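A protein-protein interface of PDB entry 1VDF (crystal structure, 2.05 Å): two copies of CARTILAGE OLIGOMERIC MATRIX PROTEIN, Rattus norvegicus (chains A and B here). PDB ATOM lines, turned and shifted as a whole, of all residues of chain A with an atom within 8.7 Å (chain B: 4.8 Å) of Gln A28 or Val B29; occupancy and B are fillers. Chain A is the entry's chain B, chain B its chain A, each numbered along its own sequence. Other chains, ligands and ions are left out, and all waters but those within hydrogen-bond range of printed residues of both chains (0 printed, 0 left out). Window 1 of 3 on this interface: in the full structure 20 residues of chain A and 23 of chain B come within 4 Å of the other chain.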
ATOM      1  N   ASP A  20      18.887 -20.132  32.544  1.00  0.00           N
ATOM      2  CA  ASP A  20      18.658 -20.972  31.373  1.00  0.00           C
ATOM      3  C   ASP A  20      17.294 -21.635  31.398  1.00  0.00           C
ATOM      4  O   ASP A  20      16.583 -21.655  30.392  1.00  0.00           O
ATOM      5  CB  ASP A  20      19.770 -22.009  31.189  1.00  0.00           C
ATOM      6  CG  ASP A  20      20.280 -22.066  29.758  1.00  0.00           C
ATOM      7  OD1 ASP A  20      21.052 -21.186  29.341  1.00  0.00           O
ATOM      8  OD2 ASP A  20      19.854 -23.039  29.028  1.00  0.00           O
ATOM      9  N   VAL A  21      16.942 -22.179  32.559  1.00  0.00           N
ATOM     10  CA  VAL A  21      15.659 -22.842  32.764  1.00  0.00           C
ATOM     11  C   VAL A  21      14.480 -21.895  32.464  1.00  0.00           C
ATOM     12  O   VAL A  21      13.491 -22.320  31.901  1.00  0.00           O
ATOM     13  CB  VAL A  21      15.528 -23.377  34.200  1.00  0.00           C
ATOM     14  CG1 VAL A  21      14.068 -23.654  34.572  1.00  0.00           C
ATOM     15  CG2 VAL A  21      16.393 -24.622  34.395  1.00  0.00           C
ATOM     16  N   ARG A  22      14.548 -20.625  32.884  1.00  0.00           N
ATOM     17  CA  ARG A  22      13.422 -19.726  32.626  1.00  0.00           C
ATOM     18  C   ARG A  22      13.405 -19.373  31.143  1.00  0.00           C
ATOM     19  O   ARG A  22      12.344 -19.250  30.522  1.00  0.00           O
ATOM     20  CB  ARG A  22      13.463 -18.484  33.524  1.00  0.00           C
ATOM     21  CG  ARG A  22      13.708 -17.189  32.811  1.00  0.00           C
ATOM     22  CD  ARG A  22      13.586 -16.006  33.763  1.00  0.00           C
ATOM     23  NE  ARG A  22      14.678 -15.053  33.615  1.00  0.00           N
ATOM     24  CZ  ARG A  22      15.058 -14.209  34.570  1.00  0.00           C
ATOM     25  NH1 ARG A  22      14.449 -14.207  35.746  1.00  0.00           N
ATOM     26  NH2 ARG A  22      16.055 -13.366  34.343  1.00  0.00           N
ATOM     27  N   GLU A  23      14.593 -19.276  30.561  1.00  0.00           N
ATOM     28  CA  GLU A  23      14.686 -19.005  29.134  1.00  0.00           C
ATOM     29  C   GLU A  23      14.079 -20.182  28.355  1.00  0.00           C
ATOM     30  O   GLU A  23      13.343 -20.010  27.362  1.00  0.00           O
ATOM     31  CB  GLU A  23      16.158 -18.803  28.713  1.00  0.00           C
ATOM     32  CG  GLU A  23      16.316 -18.146  27.315  1.00  0.00           C
ATOM     33  CD  GLU A  23      17.090 -19.003  26.343  1.00  0.00           C
ATOM     34  OE1 GLU A  23      17.305 -20.218  26.686  1.00  0.00           O
ATOM     35  OE2 GLU A  23      17.467 -18.526  25.272  1.00  0.00           O
ATOM     36  N   LEU A  24      14.415 -21.382  28.805  1.00  0.00           N
ATOM     37  CA  LEU A  24      13.926 -22.587  28.162  1.00  0.00           C
ATOM     38  C   LEU A  24      12.428 -22.707  28.299  1.00  0.00           C
ATOM     39  O   LEU A  24      11.738 -23.032  27.329  1.00  0.00           O
ATOM     40  CB  LEU A  24      14.636 -23.811  28.709  1.00  0.00           C
ATOM     41  CG  LEU A  24      16.051 -23.940  28.112  1.00  0.00           C
ATOM     42  CD1 LEU A  24      16.884 -24.974  28.900  1.00  0.00           C
ATOM     43  CD2 LEU A  24      16.017 -24.311  26.627  1.00  0.00           C
ATOM     44  N   LEU A  25      11.926 -22.416  29.492  1.00  0.00           N
ATOM     45  CA  LEU A  25      10.501 -22.461  29.756  1.00  0.00           C
ATOM     46  C   LEU A  25       9.778 -21.408  28.947  1.00  0.00           C
ATOM     47  O   LEU A  25       8.655 -21.630  28.516  1.00  0.00           O
ATOM     48  CB  LEU A  25      10.180 -22.281  31.262  1.00  0.00           C
ATOM     49  CG  LEU A  25      10.282 -23.554  32.096  1.00  0.00           C
ATOM     50  CD1 LEU A  25       9.927 -23.186  33.514  1.00  0.00           C
ATOM     51  CD2 LEU A  25       9.313 -24.621  31.575  1.00  0.00           C
ATOM     52  N   ARG A  26      10.419 -20.267  28.720  1.00  0.00           N
ATOM     53  CA  ARG A  26       9.763 -19.238  27.919  1.00  0.00           C
ATOM     54  C   ARG A  26       9.560 -19.720  26.482  1.00  0.00           C
ATOM     55  O   ARG A  26       8.515 -19.504  25.861  1.00  0.00           O
ATOM     56  CB  ARG A  26      10.587 -17.967  27.871  1.00  0.00           C
ATOM     57  CG  ARG A  26      10.468 -17.042  29.092  1.00  0.00           C
ATOM     58  CD  ARG A  26      11.301 -15.767  28.911  1.00  0.00           C
ATOM     59  NE  ARG A  26      12.739 -15.965  29.062  1.00  0.00           N
ATOM     60  CZ  ARG A  26      13.522 -15.206  29.829  1.00  0.00           C
ATOM     61  NH1 ARG A  26      12.991 -14.190  30.490  1.00  0.00           N
ATOM     62  NH2 ARG A  26      14.823 -15.466  29.938  1.00  0.00           N
ATOM     63  N   GLN A  27      10.586 -20.359  25.955  1.00  0.00           N
ATOM     64  CA  GLN A  27      10.538 -20.894  24.592  1.00  0.00           C
ATOM     65  C   GLN A  27       9.522 -22.013  24.483  1.00  0.00           C
ATOM     66  O   GLN A  27       8.894 -22.216  23.436  1.00  0.00           O
ATOM     67  CB  GLN A  27      11.936 -21.425  24.224  1.00  0.00           C
ATOM     68  CG  GLN A  27      12.047 -22.220  22.916  1.00  0.00           C
ATOM     69  CD  GLN A  27      13.494 -22.610  22.626  1.00  0.00           C
ATOM     70  OE1 GLN A  27      14.383 -22.423  23.474  1.00  0.00           O
ATOM     71  NE2 GLN A  27      13.742 -23.140  21.429  1.00  0.00           N
ATOM     72  N   GLN A  28       9.367 -22.760  25.566  1.00  0.00           N
ATOM     73  CA  GLN A  28       8.459 -23.897  25.549  1.00  0.00           C
ATOM     74  C   GLN A  28       7.012 -23.455  25.579  1.00  0.00           C
ATOM     75  O   GLN A  28       6.166 -23.985  24.881  1.00  0.00           O
ATOM     76  CB  GLN A  28       8.784 -24.830  26.717  1.00  0.00           C
ATOM     77  CG  GLN A  28       8.270 -26.254  26.558  1.00  0.00           C
ATOM     78  CD  GLN A  28       8.666 -27.126  27.726  1.00  0.00           C
ATOM     79  OE1 GLN A  28       9.560 -27.951  27.616  1.00  0.00           O
ATOM     80  NE2 GLN A  28       8.018 -26.918  28.872  1.00  0.00           N
ATOM     81  N   VAL A  29       6.727 -22.451  26.376  1.00  0.00           N
ATOM     82  CA  VAL A  29       5.367 -21.938  26.457  1.00  0.00           C
ATOM     83  C   VAL A  29       4.946 -21.486  25.082  1.00  0.00           C
ATOM     84  O   VAL A  29       3.800 -21.633  24.674  1.00  0.00           O
ATOM     85  CB  VAL A  29       5.296 -20.692  27.387  1.00  0.00           C
ATOM     86  CG1 VAL A  29       3.870 -20.249  27.598  1.00  0.00           C
ATOM     87  CG2 VAL A  29       5.939 -20.979  28.724  1.00  0.00           C
ATOM     88  N   LYS A  30       5.887 -20.879  24.380  1.00  0.00           N
ATOM     89  CA  LYS A  30       5.599 -20.378  23.064  1.00  0.00           C
ATOM     90  C   LYS A  30       5.262 -21.498  22.092  1.00  0.00           C
ATOM     91  O   LYS A  30       4.379 -21.378  21.252  1.00  0.00           O
ATOM     92  CB  LYS A  30       6.758 -19.545  22.546  1.00  0.00           C
ATOM     93  CG  LYS A  30       6.328 -18.261  21.835  1.00  0.00           C
ATOM     94  CD  LYS A  30       7.515 -17.511  21.232  1.00  0.00           C
ATOM     95  CE  LYS A  30       7.060 -16.380  20.338  1.00  0.00           C
ATOM     96  NZ  LYS A  30       8.087 -16.043  19.356  1.00  0.00           N
ATOM     97  N   GLU A  31       5.997 -22.585  22.163  1.00  0.00           N
ATOM     98  CA  GLU A  31       5.727 -23.680  21.247  1.00  0.00           C
ATOM     99  C   GLU A  31       4.351 -24.268  21.548  1.00  0.00           C
ATOM    100  O   GLU A  31       3.543 -24.470  20.655  1.00  0.00           O
ATOM    101  CB  GLU A  31       6.815 -24.738  21.388  1.00  0.00           C
ATOM    102  CG  GLU A  31       8.242 -24.149  21.348  1.00  0.00           C
ATOM    103  CD  GLU A  31       8.782 -24.117  19.954  1.00  0.00           C
ATOM    104  OE1 GLU A  31       8.011 -24.333  19.015  1.00  0.00           O
ATOM    105  OE2 GLU A  31      10.039 -23.888  19.822  1.00  0.00           O
ATOM    106  N   ILE A  32       4.095 -24.510  22.831  1.00  0.00           N
ATOM    107  CA  ILE A  32       2.837 -25.069  23.302  1.00  0.00           C
ATOM    108  C   ILE A  32       1.655 -24.190  22.903  1.00  0.00           C
ATOM    109  O   ILE A  32       0.658 -24.676  22.372  1.00  0.00           O
ATOM    110  CB  ILE A  32       2.883 -25.345  24.821  1.00  0.00           C
ATOM    111  CG1 ILE A  32       3.726 -26.602  25.070  1.00  0.00           C
ATOM    112  CG2 ILE A  32       1.509 -25.584  25.406  1.00  0.00           C
ATOM    113  CD1 ILE A  32       4.439 -26.630  26.430  1.00  0.00           C
ATOM    114  N   THR A  33       1.765 -22.890  23.146  1.00  0.00           N
ATOM    115  CA  THR A  33       0.664 -22.021  22.785  1.00  0.00           C
ATOM    116  C   THR A  33       0.366 -22.153  21.290  1.00  0.00           C
ATOM    117  O   THR A  33      -0.792 -22.274  20.877  1.00  0.00           O
ATOM    118  CB  THR A  33       0.922 -20.546  23.168  1.00  0.00           C
ATOM    119  OG1 THR A  33       1.274 -20.464  24.561  1.00  0.00           O
ATOM    120  CG2 THR A  33      -0.336 -19.711  22.870  1.00  0.00           C
ATOM    121  N   PHE A  34       1.410 -22.127  20.477  1.00  0.00           N
ATOM    122  CA  PHE A  34       1.255 -22.286  19.025  1.00  0.00           C
ATOM    123  C   PHE A  34       0.609 -23.630  18.714  1.00  0.00           C
ATOM    124  O   PHE A  34      -0.268 -23.735  17.865  1.00  0.00           O
ATOM    125  CB  PHE A  34       2.611 -22.248  18.329  1.00  0.00           C
ATOM    126  CG  PHE A  34       2.515 -21.934  16.881  1.00  0.00           C
ATOM    127  CD1 PHE A  34       2.409 -20.609  16.464  1.00  0.00           C
ATOM    128  CD2 PHE A  34       2.512 -22.949  15.924  1.00  0.00           C
ATOM    129  CE1 PHE A  34       2.315 -20.290  15.111  1.00  0.00           C
ATOM    130  CE2 PHE A  34       2.398 -22.641  14.571  1.00  0.00           C
ATOM    131  CZ  PHE A  34       2.305 -21.310  14.163  1.00  0.00           C
ATOM    132  N   LEU A  35       1.059 -24.676  19.386  1.00  0.00           N
ATOM    133  CA  LEU A  35       0.461 -25.972  19.161  1.00  0.00           C
ATOM    134  C   LEU A  35      -1.043 -25.845  19.478  1.00  0.00           C
ATOM    135  O   LEU A  35      -1.887 -26.239  18.675  1.00  0.00           O
ATOM    136  CB  LEU A  35       1.148 -27.029  20.038  1.00  0.00           C
ATOM    137  CG  LEU A  35       0.650 -28.458  19.886  1.00  0.00           C
ATOM    138  CD1 LEU A  35       0.955 -28.946  18.486  1.00  0.00           C
ATOM    139  CD2 LEU A  35       1.325 -29.341  20.917  1.00  0.00           C
ATOM    140  N   LEU B  25      14.859 -30.240  30.258  1.00  0.00           N
ATOM    141  CA  LEU B  25      14.078 -29.170  29.661  1.00  0.00           C
ATOM    142  C   LEU B  25      14.534 -28.975  28.233  1.00  0.00           C
ATOM    143  O   LEU B  25      13.723 -28.770  27.316  1.00  0.00           O
ATOM    144  CB  LEU B  25      14.239 -27.847  30.424  1.00  0.00           C
ATOM    145  CG  LEU B  25      13.117 -27.456  31.382  1.00  0.00           C
ATOM    146  CD1 LEU B  25      12.817 -25.984  31.205  1.00  0.00           C
ATOM    147  CD2 LEU B  25      11.859 -28.274  31.138  1.00  0.00           C
ATOM    148  N   ARG B  26      15.842 -29.035  28.048  1.00  0.00           N
ATOM    149  CA  ARG B  26      16.410 -28.853  26.736  1.00  0.00           C
ATOM    150  C   ARG B  26      15.908 -29.893  25.735  1.00  0.00           C
ATOM    151  O   ARG B  26      15.571 -29.564  24.593  1.00  0.00           O
ATOM    152  CB  ARG B  26      17.931 -28.897  26.822  1.00  0.00           C
ATOM    153  CG  ARG B  26      18.585 -27.640  26.281  1.00  0.00           C
ATOM    154  CD  ARG B  26      20.040 -27.890  25.965  1.00  0.00           C
ATOM    155  NE  ARG B  26      20.828 -28.146  27.168  1.00  0.00           N
ATOM    156  CZ  ARG B  26      21.279 -27.200  27.992  1.00  0.00           C
ATOM    157  NH1 ARG B  26      21.013 -25.913  27.780  1.00  0.00           N
ATOM    158  NH2 ARG B  26      21.999 -27.548  29.051  1.00  0.00           N
ATOM    159  N   GLN B  27      15.866 -31.143  26.177  1.00  0.00           N
ATOM    160  CA  GLN B  27      15.394 -32.208  25.339  1.00  0.00           C
ATOM    161  C   GLN B  27      13.899 -32.040  25.157  1.00  0.00           C
ATOM    162  O   GLN B  27      13.363 -32.316  24.073  1.00  0.00           O
ATOM    163  CB  GLN B  27      15.673 -33.587  25.963  1.00  0.00           C
ATOM    164  CG  GLN B  27      15.411 -34.779  24.988  1.00  0.00           C
ATOM    165  CD  GLN B  27      15.410 -36.160  25.674  1.00  0.00           C
ATOM    166  OE1 GLN B  27      15.942 -36.320  26.782  1.00  0.00           O
ATOM    167  NE2 GLN B  27      14.822 -37.162  25.008  1.00  0.00           N
ATOM    168  N   GLN B  28      13.229 -31.605  26.226  1.00  0.00           N
ATOM    169  CA  GLN B  28      11.779 -31.437  26.199  1.00  0.00           C
ATOM    170  C   GLN B  28      11.307 -30.434  25.157  1.00  0.00           C
ATOM    171  O   GLN B  28      10.330 -30.675  24.419  1.00  0.00           O
ATOM    172  CB  GLN B  28      11.240 -31.064  27.579  1.00  0.00           C
ATOM    173  CG  GLN B  28       9.736 -31.143  27.650  1.00  0.00           C
ATOM    174  CD  GLN B  28       9.224 -31.051  29.058  1.00  0.00           C
ATOM    175  OE1 GLN B  28       9.024 -32.071  29.720  1.00  0.00           O
ATOM    176  NE2 GLN B  28       8.932 -29.840  29.496  1.00  0.00           N
ATOM    177  N   VAL B  29      11.999 -29.309  25.098  1.00  0.00           N
ATOM    178  CA  VAL B  29      11.658 -28.281  24.118  1.00  0.00           C
ATOM    179  C   VAL B  29      11.784 -28.850  22.686  1.00  0.00           C
ATOM    180  O   VAL B  29      10.946 -28.592  21.811  1.00  0.00           O
ATOM    181  CB  VAL B  29      12.566 -27.060  24.294  1.00  0.00           C
ATOM    182  CG1 VAL B  29      12.367 -26.070  23.155  1.00  0.00           C
ATOM    183  CG2 VAL B  29      12.275 -26.375  25.638  1.00  0.00           C
ATOM    184  N   LYS B  30      12.839 -29.625  22.464  1.00  0.00           N
ATOM    185  CA  LYS B  30      13.088 -30.227  21.171  1.00  0.00           C
ATOM    186  C   LYS B  30      11.992 -31.203  20.780  1.00  0.00           C
ATOM    187  O   LYS B  30      11.565 -31.216  19.648  1.00  0.00           O
ATOM    188  CB  LYS B  30      14.466 -30.882  21.110  1.00  0.00           C
ATOM    189  CG  LYS B  30      15.603 -29.906  20.804  1.00  0.00           C
ATOM    190  CD  LYS B  30      15.261 -28.468  21.210  1.00  0.00           C
ATOM    191  CE  LYS B  30      16.495 -27.668  21.652  1.00  0.00           C
ATOM    192  NZ  LYS B  30      16.402 -27.221  23.066  1.00  0.00           N
ATOM    193  N   GLU B  31      11.480 -31.975  21.729  1.00  0.00           N
ATOM    194  CA  GLU B  31      10.383 -32.890  21.412  1.00  0.00           C
ATOM    195  C   GLU B  31       9.057 -32.176  21.075  1.00  0.00           C
ATOM    196  O   GLU B  31       8.328 -32.599  20.183  1.00  0.00           O
ATOM    197  CB  GLU B  31      10.138 -33.878  22.557  1.00  0.00           C
ATOM    198  CG  GLU B  31      11.360 -34.702  22.962  1.00  0.00           C
ATOM    199  CD  GLU B  31      11.748 -35.757  21.950  1.00  0.00           C
ATOM    200  OE1 GLU B  31      11.000 -36.044  21.024  1.00  0.00           O
ATOM    201  OE2 GLU B  31      12.868 -36.344  22.154  1.00  0.00           O
ATOM    202  N   ILE B  32       8.736 -31.106  21.814  1.00  0.00           N
ATOM    203  CA  ILE B  32       7.497 -30.320  21.621  1.00  0.00           C
ATOM    204  C   ILE B  32       7.558 -29.507  20.336  1.00  0.00           C
ATOM    205  O   ILE B  32       6.570 -29.297  19.696  1.00  0.00           O
ATOM    206  CB  ILE B  32       7.255 -29.345  22.771  1.00  0.00           C
ATOM    207  CG1 ILE B  32       6.755 -30.054  23.997  1.00  0.00           C
ATOM    208  CG2 ILE B  32       6.286 -28.252  22.362  1.00  0.00           C
ATOM    209  CD1 ILE B  32       7.515 -29.559  25.226  1.00  0.00           C
ATOM    210  N   THR B  33       8.739 -29.047  19.954  1.00  0.00           N
ATOM    211  CA  THR B  33       8.855 -28.338  18.713  1.00  0.00           C
ATOM    212  C   THR B  33       8.615 -29.341  17.591  1.00  0.00           C
ATOM    213  O   THR B  33       7.924 -29.075  16.613  1.00  0.00           O
ATOM    214  CB  THR B  33      10.257 -27.772  18.566  1.00  0.00           C
ATOM    215  OG1 THR B  33      10.561 -27.019  19.722  1.00  0.00           O
ATOM    216  CG2 THR B  33      10.354 -26.889  17.328  1.00  0.00           C
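Leu B25 touches its own counterpart, Leu A25.
Gln A27 touches Val B29, but with the chains exchanged Val A29 does not touch Gln B27 (12.0 Å).
Gln B28 touches its own counterpart, Gln A28.
Gln A28 touches Val B29, but with the chains exchanged Val A29 does not touch Gln B28 (8.3 Å).
Positions printed for both chains: 25, 26, 27, 28, 29, 30, 31, 32 and 33.
Of the 11 pairs that touch across the chains among the printed residues, 2 have their exchanged pair printed and touching as well.
The side-chain carboxylate (OD2) of Asp A20 is in salt-bridge range of the guanidinium group (NH1) of Arg B26, at 3.3 Å.
The side-chain amide oxygen (OE1) of Gln A28 is in hydrogen-bond range of the side-chain amide nitrogen (NE2) of Gln B28, at 2.7 Å.
OG1 of Thr B33 sits at hydrogen-bond distance from OE2 of Glu A31, at 3.2 Å.
The side-chain amino group (NZ) of Lys B30 lies within hydrogen-bond range of the backbone carbonyl oxygen (O) of Arg B26.
OG1 of Thr B33 is in hydrogen-bond range of O of Val B29 (2.6 Å).
Among the printed residues, pairs that only touch across the chains: Val A21 with Leu B25, Leu A24 with Leu B25, Leu A24 with Val B29, Leu A25 with Leu B25, Gln A27 with Val B29, Gln A28 with Val B29, Gln A28 with Ile B32 and Glu A31 with Ile B32.
Of the printed residues of chain B, Asp A20 touches Arg B26.
Of the printed residues of chain B, Leu A24 touches Leu B25 (3.8 Å) and Val B29 (3.8 Å).
Printed residues of chain B within 4 Å of Leu A25: Leu B25.
Gln A28 touches three residues of chain B.
Printed residues of chain B within 4 Å of Glu A31: Ile B32 and Thr B33.
Val B29 touches just these residues of chain A: Leu A24, Gln A27 and Gln A28.
The nearest residue of chain B that does not touch Gln A28 is Leu B25 (4.2 Å).
The nearest residue of chain A that does not touch Val B29 is Glu A31 (4.6 Å).
Hydrophobic or aromatic side chains of chain A within 4 Å of the printed part of chain B: Leu A24 and Leu A25.
Of the 9 printed residues of chain B, 6 touch a printed residue of chain A.
Among the printed residues, 11 pairs touch across the chains.
Among the printed residues, Asp or Glu carboxylates within 4 Å of a Lys or Arg side-chain nitrogen of the other chain: Asp A20 with Arg B26.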
